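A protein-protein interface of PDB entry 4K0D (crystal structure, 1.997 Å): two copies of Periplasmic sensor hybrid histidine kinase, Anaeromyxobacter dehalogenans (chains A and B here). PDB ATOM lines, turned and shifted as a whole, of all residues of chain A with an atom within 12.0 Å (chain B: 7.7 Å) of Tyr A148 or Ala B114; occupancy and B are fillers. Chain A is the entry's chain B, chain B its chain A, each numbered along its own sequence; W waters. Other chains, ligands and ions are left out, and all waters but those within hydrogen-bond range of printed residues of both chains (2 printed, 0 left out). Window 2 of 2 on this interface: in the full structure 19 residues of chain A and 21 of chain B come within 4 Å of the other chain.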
ATOM      1  N   ILE A   5      16.675 -22.561   9.544  1.00  0.00           N
ATOM      2  CA  ILE A   5      18.061 -22.723   9.113  1.00  0.00           C
ATOM      3  C   ILE A   5      18.099 -22.998   7.614  1.00  0.00           C
ATOM      4  O   ILE A   5      18.658 -24.008   7.153  1.00  0.00           O
ATOM      5  CB  ILE A   5      18.777 -23.859   9.875  1.00  0.00           C
ATOM      6  N   GLY A 140      14.801  -9.105  16.948  1.00  0.00           N
ATOM      7  CA  GLY A 140      13.650 -10.006  16.996  1.00  0.00           C
ATOM      8  C   GLY A 140      13.682 -11.006  15.834  1.00  0.00           C
ATOM      9  O   GLY A 140      13.272 -12.160  15.979  1.00  0.00           O
ATOM     10  N   ALA A 141      14.157 -10.598  14.661  1.00  0.00           N
ATOM     11  CA  ALA A 141      14.139 -11.525  13.540  1.00  0.00           C
ATOM     12  C   ALA A 141      15.227 -12.570  13.750  1.00  0.00           C
ATOM     13  O   ALA A 141      15.025 -13.748  13.536  1.00  0.00           O
ATOM     14  CB  ALA A 141      14.331 -10.796  12.242  1.00  0.00           C
ATOM     15  N   SER A 142      16.400 -12.131  14.166  1.00  0.00           N
ATOM     16  CA  SER A 142      17.465 -13.060  14.495  1.00  0.00           C
ATOM     17  C   SER A 142      17.024 -14.076  15.521  1.00  0.00           C
ATOM     18  O   SER A 142      17.276 -15.278  15.372  1.00  0.00           O
ATOM     19  CB  SER A 142      18.636 -12.309  15.059  1.00  0.00           C
ATOM     20  OG  SER A 142      19.077 -11.473  14.041  1.00  0.00           O
ATOM     21  N   HIS A 143      16.403 -13.589  16.586  1.00  0.00           N
ATOM     22  CA  HIS A 143      16.009 -14.482  17.646  1.00  0.00           C
ATOM     23  C   HIS A 143      15.119 -15.571  17.100  1.00  0.00           C
ATOM     24  O   HIS A 143      15.307 -16.751  17.410  1.00  0.00           O
ATOM     25  CB  HIS A 143      15.273 -13.765  18.759  1.00  0.00           C
ATOM     26  CG  HIS A 143      14.945 -14.675  19.894  1.00  0.00           C
ATOM     27  ND1 HIS A 143      15.855 -14.986  20.877  1.00  0.00           N
ATOM     28  CD2 HIS A 143      13.828 -15.399  20.165  1.00  0.00           C
ATOM     29  CE1 HIS A 143      15.303 -15.833  21.736  1.00  0.00           C
ATOM     30  NE2 HIS A 143      14.075 -16.090  21.326  1.00  0.00           N
ATOM     31  N   THR A 144      14.141 -15.161  16.298  1.00  0.00           N
ATOM     32  CA  THR A 144      13.121 -16.055  15.792  1.00  0.00           C
ATOM     33  C   THR A 144      13.789 -17.032  14.860  1.00  0.00           C
ATOM     34  O   THR A 144      13.538 -18.227  14.887  1.00  0.00           O
ATOM     35  CB  THR A 144      12.076 -15.265  15.014  1.00  0.00           C
ATOM     36  OG1 THR A 144      11.263 -14.530  15.933  1.00  0.00           O
ATOM     37  CG2 THR A 144      11.198 -16.183  14.180  1.00  0.00           C
ATOM     38  N   ILE A 145      14.688 -16.519  14.027  1.00  0.00           N
ATOM     39  CA  ILE A 145      15.359 -17.408  13.108  1.00  0.00           C
ATOM     40  C   ILE A 145      16.178 -18.444  13.853  1.00  0.00           C
ATOM     41  O   ILE A 145      16.267 -19.579  13.416  1.00  0.00           O
ATOM     42  CB  ILE A 145      16.255 -16.658  12.101  1.00  0.00           C
ATOM     43  CG1 ILE A 145      15.384 -16.137  10.962  1.00  0.00           C
ATOM     44  CG2 ILE A 145      17.312 -17.612  11.538  1.00  0.00           C
ATOM     45  CD1 ILE A 145      16.043 -15.018  10.214  1.00  0.00           C
ATOM     46  N   LEU A 146      16.810 -18.087  14.960  1.00  0.00           N
ATOM     47  CA  LEU A 146      17.591 -19.097  15.654  1.00  0.00           C
ATOM     48  C   LEU A 146      16.789 -19.860  16.714  1.00  0.00           C
ATOM     49  O   LEU A 146      17.383 -20.535  17.539  1.00  0.00           O
ATOM     50  CB  LEU A 146      18.821 -18.474  16.291  1.00  0.00           C
ATOM     51  CG  LEU A 146      19.686 -17.645  15.330  1.00  0.00           C
ATOM     52  CD1 LEU A 146      20.822 -16.986  16.057  1.00  0.00           C
ATOM     53  CD2 LEU A 146      20.232 -18.538  14.279  1.00  0.00           C
ATOM     54  N   ALA A 147      15.462 -19.736  16.728  1.00  0.00           N
ATOM     55  CA  ALA A 147      14.685 -20.379  17.771  1.00  0.00           C
ATOM     56  C   ALA A 147      14.663 -21.913  17.516  1.00  0.00           C
ATOM     57  O   ALA A 147      14.730 -22.345  16.364  1.00  0.00           O
ATOM     58  CB  ALA A 147      13.262 -19.813  17.811  1.00  0.00           C
ATOM     59  N   TYR A 148      14.598 -22.708  18.591  1.00  0.00           N
ATOM     60  CA  TYR A 148      14.510 -24.182  18.493  1.00  0.00           C
ATOM     61  C   TYR A 148      13.134 -24.648  18.002  1.00  0.00           C
ATOM     62  O   TYR A 148      12.105 -24.141  18.466  1.00  0.00           O
ATOM     63  CB  TYR A 148      14.794 -24.829  19.846  1.00  0.00           C
ATOM     64  CG  TYR A 148      16.231 -24.712  20.272  1.00  0.00           C
ATOM     65  CD1 TYR A 148      17.234 -25.384  19.575  1.00  0.00           C
ATOM     66  CD2 TYR A 148      16.603 -23.934  21.374  1.00  0.00           C
ATOM     67  CE1 TYR A 148      18.571 -25.281  19.967  1.00  0.00           C
ATOM     68  CE2 TYR A 148      17.948 -23.827  21.780  1.00  0.00           C
ATOM     69  CZ  TYR A 148      18.921 -24.507  21.065  1.00  0.00           C
ATOM     70  OH  TYR A 148      20.253 -24.424  21.423  1.00  0.00           O
ATOM     71  N   GLN A 149      13.115 -25.605  17.069  1.00  0.00           N
ATOM     72  CA  GLN A 149      11.851 -26.075  16.467  1.00  0.00           C
ATOM     73  C   GLN A 149      11.402 -27.431  17.026  1.00  0.00           C
ATOM     74  O   GLN A 149      12.130 -28.081  17.777  1.00  0.00           O
ATOM     75  CB  GLN A 149      11.968 -26.173  14.939  1.00  0.00           C
ATOM     76  N   ARG B  38      24.508 -24.090  14.084  1.00  0.00           N
ATOM     77  CA  ARG B  38      23.238 -24.789  14.200  1.00  0.00           C
ATOM     78  C   ARG B  38      23.019 -25.631  12.938  1.00  0.00           C
ATOM     79  O   ARG B  38      22.566 -26.764  13.015  1.00  0.00           O
ATOM     80  CB  ARG B  38      22.093 -23.801  14.428  1.00  0.00           C
ATOM     81  CG  ARG B  38      20.666 -24.372  14.403  1.00  0.00           C
ATOM     82  CD  ARG B  38      20.280 -25.125  15.700  1.00  0.00           C
ATOM     83  NE  ARG B  38      20.588 -24.320  16.847  1.00  0.00           N
ATOM     84  CZ  ARG B  38      19.796 -23.350  17.303  1.00  0.00           C
ATOM     85  NH1 ARG B  38      18.613 -23.113  16.736  1.00  0.00           N
ATOM     86  NH2 ARG B  38      20.180 -22.631  18.343  1.00  0.00           N
ATOM     87  N   LEU B  96      31.512 -27.776  19.303  1.00  0.00           N
ATOM     88  CA  LEU B  96      30.335 -28.281  18.612  1.00  0.00           C
ATOM     89  C   LEU B  96      30.766 -28.927  17.314  1.00  0.00           C
ATOM     90  O   LEU B  96      30.408 -30.083  17.045  1.00  0.00           O
ATOM     91  CB  LEU B  96      29.338 -27.196  18.277  1.00  0.00           C
ATOM     92  CG  LEU B  96      28.213 -27.763  17.407  1.00  0.00           C
ATOM     93  CD1 LEU B  96      27.362 -28.806  18.151  1.00  0.00           C
ATOM     94  CD2 LEU B  96      27.296 -26.701  16.869  1.00  0.00           C
ATOM     95  N   ALA B 108      25.203 -35.816  22.329  1.00  0.00           N
ATOM     96  CA  ALA B 108      26.351 -34.993  22.657  1.00  0.00           C
ATOM     97  C   ALA B 108      26.351 -33.735  21.775  1.00  0.00           C
ATOM     98  O   ALA B 108      26.766 -32.669  22.194  1.00  0.00           O
ATOM     99  CB  ALA B 108      27.630 -35.770  22.470  1.00  0.00           C
ATOM    100  N   ILE B 109      25.889 -33.871  20.546  1.00  0.00           N
ATOM    101  CA  ILE B 109      25.785 -32.718  19.675  1.00  0.00           C
ATOM    102  C   ILE B 109      24.811 -31.719  20.293  1.00  0.00           C
ATOM    103  O   ILE B 109      25.086 -30.503  20.331  1.00  0.00           O
ATOM    104  CB  ILE B 109      25.328 -33.163  18.268  1.00  0.00           C
ATOM    105  CG1 ILE B 109      26.494 -33.871  17.553  1.00  0.00           C
ATOM    106  CG2 ILE B 109      24.858 -31.981  17.456  1.00  0.00           C
ATOM    107  CD1 ILE B 109      26.089 -34.621  16.283  1.00  0.00           C
ATOM    108  N   ARG B 110      23.686 -32.233  20.821  1.00  0.00           N
ATOM    109  CA  ARG B 110      22.631 -31.370  21.380  1.00  0.00           C
ATOM    110  C   ARG B 110      23.227 -30.606  22.540  1.00  0.00           C
ATOM    111  O   ARG B 110      23.106 -29.404  22.601  1.00  0.00           O
ATOM    112  CB  ARG B 110      21.369 -32.183  21.796  1.00  0.00           C
ATOM    113  N   ALA B 111      23.937 -31.301  23.422  1.00  0.00           N
ATOM    114  CA  ALA B 111      24.566 -30.655  24.567  1.00  0.00           C
ATOM    115  C   ALA B 111      25.651 -29.625  24.220  1.00  0.00           C
ATOM    116  O   ALA B 111      25.788 -28.645  24.928  1.00  0.00           O
ATOM    117  CB  ALA B 111      25.172 -31.658  25.452  1.00  0.00           C
ATOM    118  N   ARG B 112      26.463 -29.877  23.204  1.00  0.00           N
ATOM    119  CA  ARG B 112      27.503 -28.915  22.834  1.00  0.00           C
ATOM    120  C   ARG B 112      26.820 -27.663  22.332  1.00  0.00           C
ATOM    121  O   ARG B 112      27.224 -26.571  22.672  1.00  0.00           O
ATOM    122  CB  ARG B 112      28.418 -29.432  21.732  1.00  0.00           C
ATOM    123  CG  ARG B 112      29.400 -30.478  22.200  1.00  0.00           C
ATOM    124  CD  ARG B 112      30.345 -29.910  23.226  1.00  0.00           C
ATOM    125  N   GLU B 113      25.770 -27.854  21.535  1.00  0.00           N
ATOM    126  CA  GLU B 113      25.159 -26.770  20.813  1.00  0.00           C
ATOM    127  C   GLU B 113      24.340 -25.912  21.746  1.00  0.00           C
ATOM    128  O   GLU B 113      24.267 -24.688  21.551  1.00  0.00           O
ATOM    129  CB  GLU B 113      24.286 -27.306  19.692  1.00  0.00           C
ATOM    130  CG  GLU B 113      23.873 -26.233  18.701  1.00  0.00           C
ATOM    131  CD  GLU B 113      22.768 -25.324  19.246  1.00  0.00           C
ATOM    132  OE1 GLU B 113      21.971 -25.812  20.107  1.00  0.00           O
ATOM    133  OE2 GLU B 113      22.712 -24.129  18.813  1.00  0.00           O
ATOM    134  N   ALA B 114      23.764 -26.530  22.780  1.00  0.00           N
ATOM    135  CA  ALA B 114      22.930 -25.800  23.744  1.00  0.00           C
ATOM    136  C   ALA B 114      23.714 -24.762  24.517  1.00  0.00           C
ATOM    137  O   ALA B 114      23.143 -23.896  25.158  1.00  0.00           O
ATOM    138  CB  ALA B 114      22.281 -26.742  24.733  1.00  0.00           C
ATOM    139  N   THR B 115      25.028 -24.890  24.487  1.00  0.00           N
ATOM    140  CA  THR B 115      25.886 -23.970  25.177  1.00  0.00           C
ATOM    141  C   THR B 115      25.932 -22.606  24.475  1.00  0.00           C
ATOM    142  O   THR B 115      26.220 -21.611  25.096  1.00  0.00           O
ATOM    143  CB  THR B 115      27.294 -24.554  25.191  1.00  0.00           C
ATOM    144  OG1 THR B 115      27.316 -25.706  26.040  1.00  0.00           O
ATOM    145  CG2 THR B 115      28.255 -23.566  25.702  1.00  0.00           C
ATOM    146  N   LEU B 116      25.615 -22.556  23.192  1.00  0.00           N
ATOM    147  CA  LEU B 116      25.962 -21.402  22.387  1.00  0.00           C
ATOM    148  C   LEU B 116      25.002 -20.226  22.542  1.00  0.00           C
ATOM    149  O   LEU B 116      25.439 -19.083  22.667  1.00  0.00           O
ATOM    150  CB  LEU B 116      26.070 -21.797  20.907  1.00  0.00           C
ATOM    151  CG  LEU B 116      27.177 -22.824  20.596  1.00  0.00           C
ATOM    152  CD1 LEU B 116      27.085 -23.290  19.176  1.00  0.00           C
ATOM    153  CD2 LEU B 116      28.525 -22.165  20.845  1.00  0.00           C
ATOM    154  N   PRO B 117      23.696 -20.492  22.518  1.00  0.00           N
ATOM    155  CA  PRO B 117      22.740 -19.384  22.501  1.00  0.00           C
ATOM    156  C   PRO B 117      22.871 -18.484  23.737  1.00  0.00           C
ATOM    157  O   PRO B 117      22.828 -17.278  23.567  1.00  0.00           O
ATOM    158  CB  PRO B 117      21.379 -20.089  22.429  1.00  0.00           C
ATOM    159  CG  PRO B 117      21.701 -21.367  21.785  1.00  0.00           C
ATOM    160  CD  PRO B 117      23.025 -21.781  22.345  1.00  0.00           C
ATOM    161  N   PRO B 118      23.036 -19.048  24.956  1.00  0.00           N
ATOM    162  CA  PRO B 118      23.255 -18.061  26.042  1.00  0.00           C
ATOM    163  C   PRO B 118      24.484 -17.170  25.770  1.00  0.00           C
ATOM    164  O   PRO B 118      24.550 -16.037  26.196  1.00  0.00           O
ATOM    165  CB  PRO B 118      23.494 -18.923  27.278  1.00  0.00           C
ATOM    166  CG  PRO B 118      22.783 -20.292  26.938  1.00  0.00           C
ATOM    167  CD  PRO B 118      22.864 -20.439  25.441  1.00  0.00           C
ATOM    168  N   MET B 119      25.492 -17.696  25.110  1.00  0.00           N
ATOM    169  CA  MET B 119      26.694 -16.882  24.938  1.00  0.00           C
ATOM    170  C   MET B 119      26.447 -15.875  23.839  1.00  0.00           C
ATOM    171  O   MET B 119      26.836 -14.703  23.933  1.00  0.00           O
ATOM    172  CB  MET B 119      27.862 -17.763  24.604  1.00  0.00           C
ATOM    173  CG  MET B 119      28.333 -18.545  25.794  1.00  0.00           C
ATOM    174  SD  MET B 119      29.583 -19.969  25.153  1.00  0.00           S
ATOM    175  CE  MET B 119      31.088 -19.524  26.217  1.00  0.00           C
ATOM    176  N   ARG B 120      25.694 -16.309  22.844  1.00  0.00           N
ATOM    177  CA  ARG B 120      25.361 -15.456  21.740  1.00  0.00           C
ATOM    178  C   ARG B 120      24.568 -14.297  22.274  1.00  0.00           C
ATOM    179  O   ARG B 120      24.850 -13.205  21.937  1.00  0.00           O
ATOM    180  CB  ARG B 120      24.530 -16.210  20.730  1.00  0.00           C
ATOM    181  CG  ARG B 120      23.963 -15.369  19.653  1.00  0.00           C
ATOM    182  CD  ARG B 120      23.045 -16.201  18.861  1.00  0.00           C
ATOM    183  NE  ARG B 120      21.665 -16.080  19.309  1.00  0.00           N
ATOM    184  CZ  ARG B 120      20.847 -17.107  19.531  1.00  0.00           C
ATOM    185  NH1 ARG B 120      21.254 -18.355  19.375  1.00  0.00           N
ATOM    186  NH2 ARG B 120      19.606 -16.883  19.889  1.00  0.00           N
HETATM  187  O   HOH W   1      18.903 -20.113  19.766  1.00  0.00           O
HETATM  188  O   HOH W   2      16.954 -18.132  19.641  1.00  0.00           O
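The side-chain hydroxyl (OH) of Tyr A148 lies within hydrogen-bond range of the side-chain carboxylate (OE1) of Glu B113 (2.6 Å). The guanidinium group (NH1) of Arg B38 is in hydrogen-bond range of the backbone carbonyl oxygen (O) of Leu A146.
NE of Arg B38 is in salt-bridge range of OE2 of Glu B113 (2.9 Å).
CD1 of Leu A146 touches CZ of Arg B120, 3.5 Å away. Ala A147 touches Arg B38 (O to NH1, 3.98 Å). NH2 of Arg B38 touches CE1 of Tyr A148, at 3.5 Å. Tyr A148 touches Ala B114. OH of Tyr A148 touches CG of Pro B117, at 3.4 Å.
Printed residues of chain B within 4 Å of Leu A146: Arg B38 (3.0 Å) and Arg B120 (3.5 Å). Ala A147 touches just one residue of chain B: Arg B38. Of chain B, only Arg B38, Glu B113, Ala B114 and Pro B117 come within 4 Å of Tyr A148. No residue of chain B comes within 4 Å of Gln A149. Printed residues of chain A within 4 Å of Arg B38: Leu A146 (3.0 Å), Ala A147 (3.98 Å) and Tyr A148 (3.5 Å). No residue of chain A comes within 4 Å of Ala B111. Of chain A, only Tyr A148 comes within 4 Å of Glu B113. Ala B114 touches just one residue of chain A: Tyr A148 (3.8 Å). Thr B115 touches none of the printed residues of chain A. No residue of chain A comes within 4 Å of Leu B116. Printed residues of chain A within 4 Å of Arg B120: Leu A146. The nearest residue of chain B that does not touch Tyr A148 is Thr B115 (5.7 Å).
Hydrophobic or aromatic side chains of chain A within 4 Å of the printed part of chain B: Leu A146 and Tyr A148. Among the printed residues, no Asp or Glu carboxylate lies within 4 Å of a Lys or Arg side-chain nitrogen of the other chain.
No position is printed for both chains.
Water W1 lies within hydrogen-bond range of O of Leu A146 (2.7 Å), NH1 of Arg B120 (3.0 Å) and NH2 of Arg B38 (3.2 Å). Water W2 lies within hydrogen-bond range of NH2 of Arg B120, O of His A143 and O of Leu A146.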
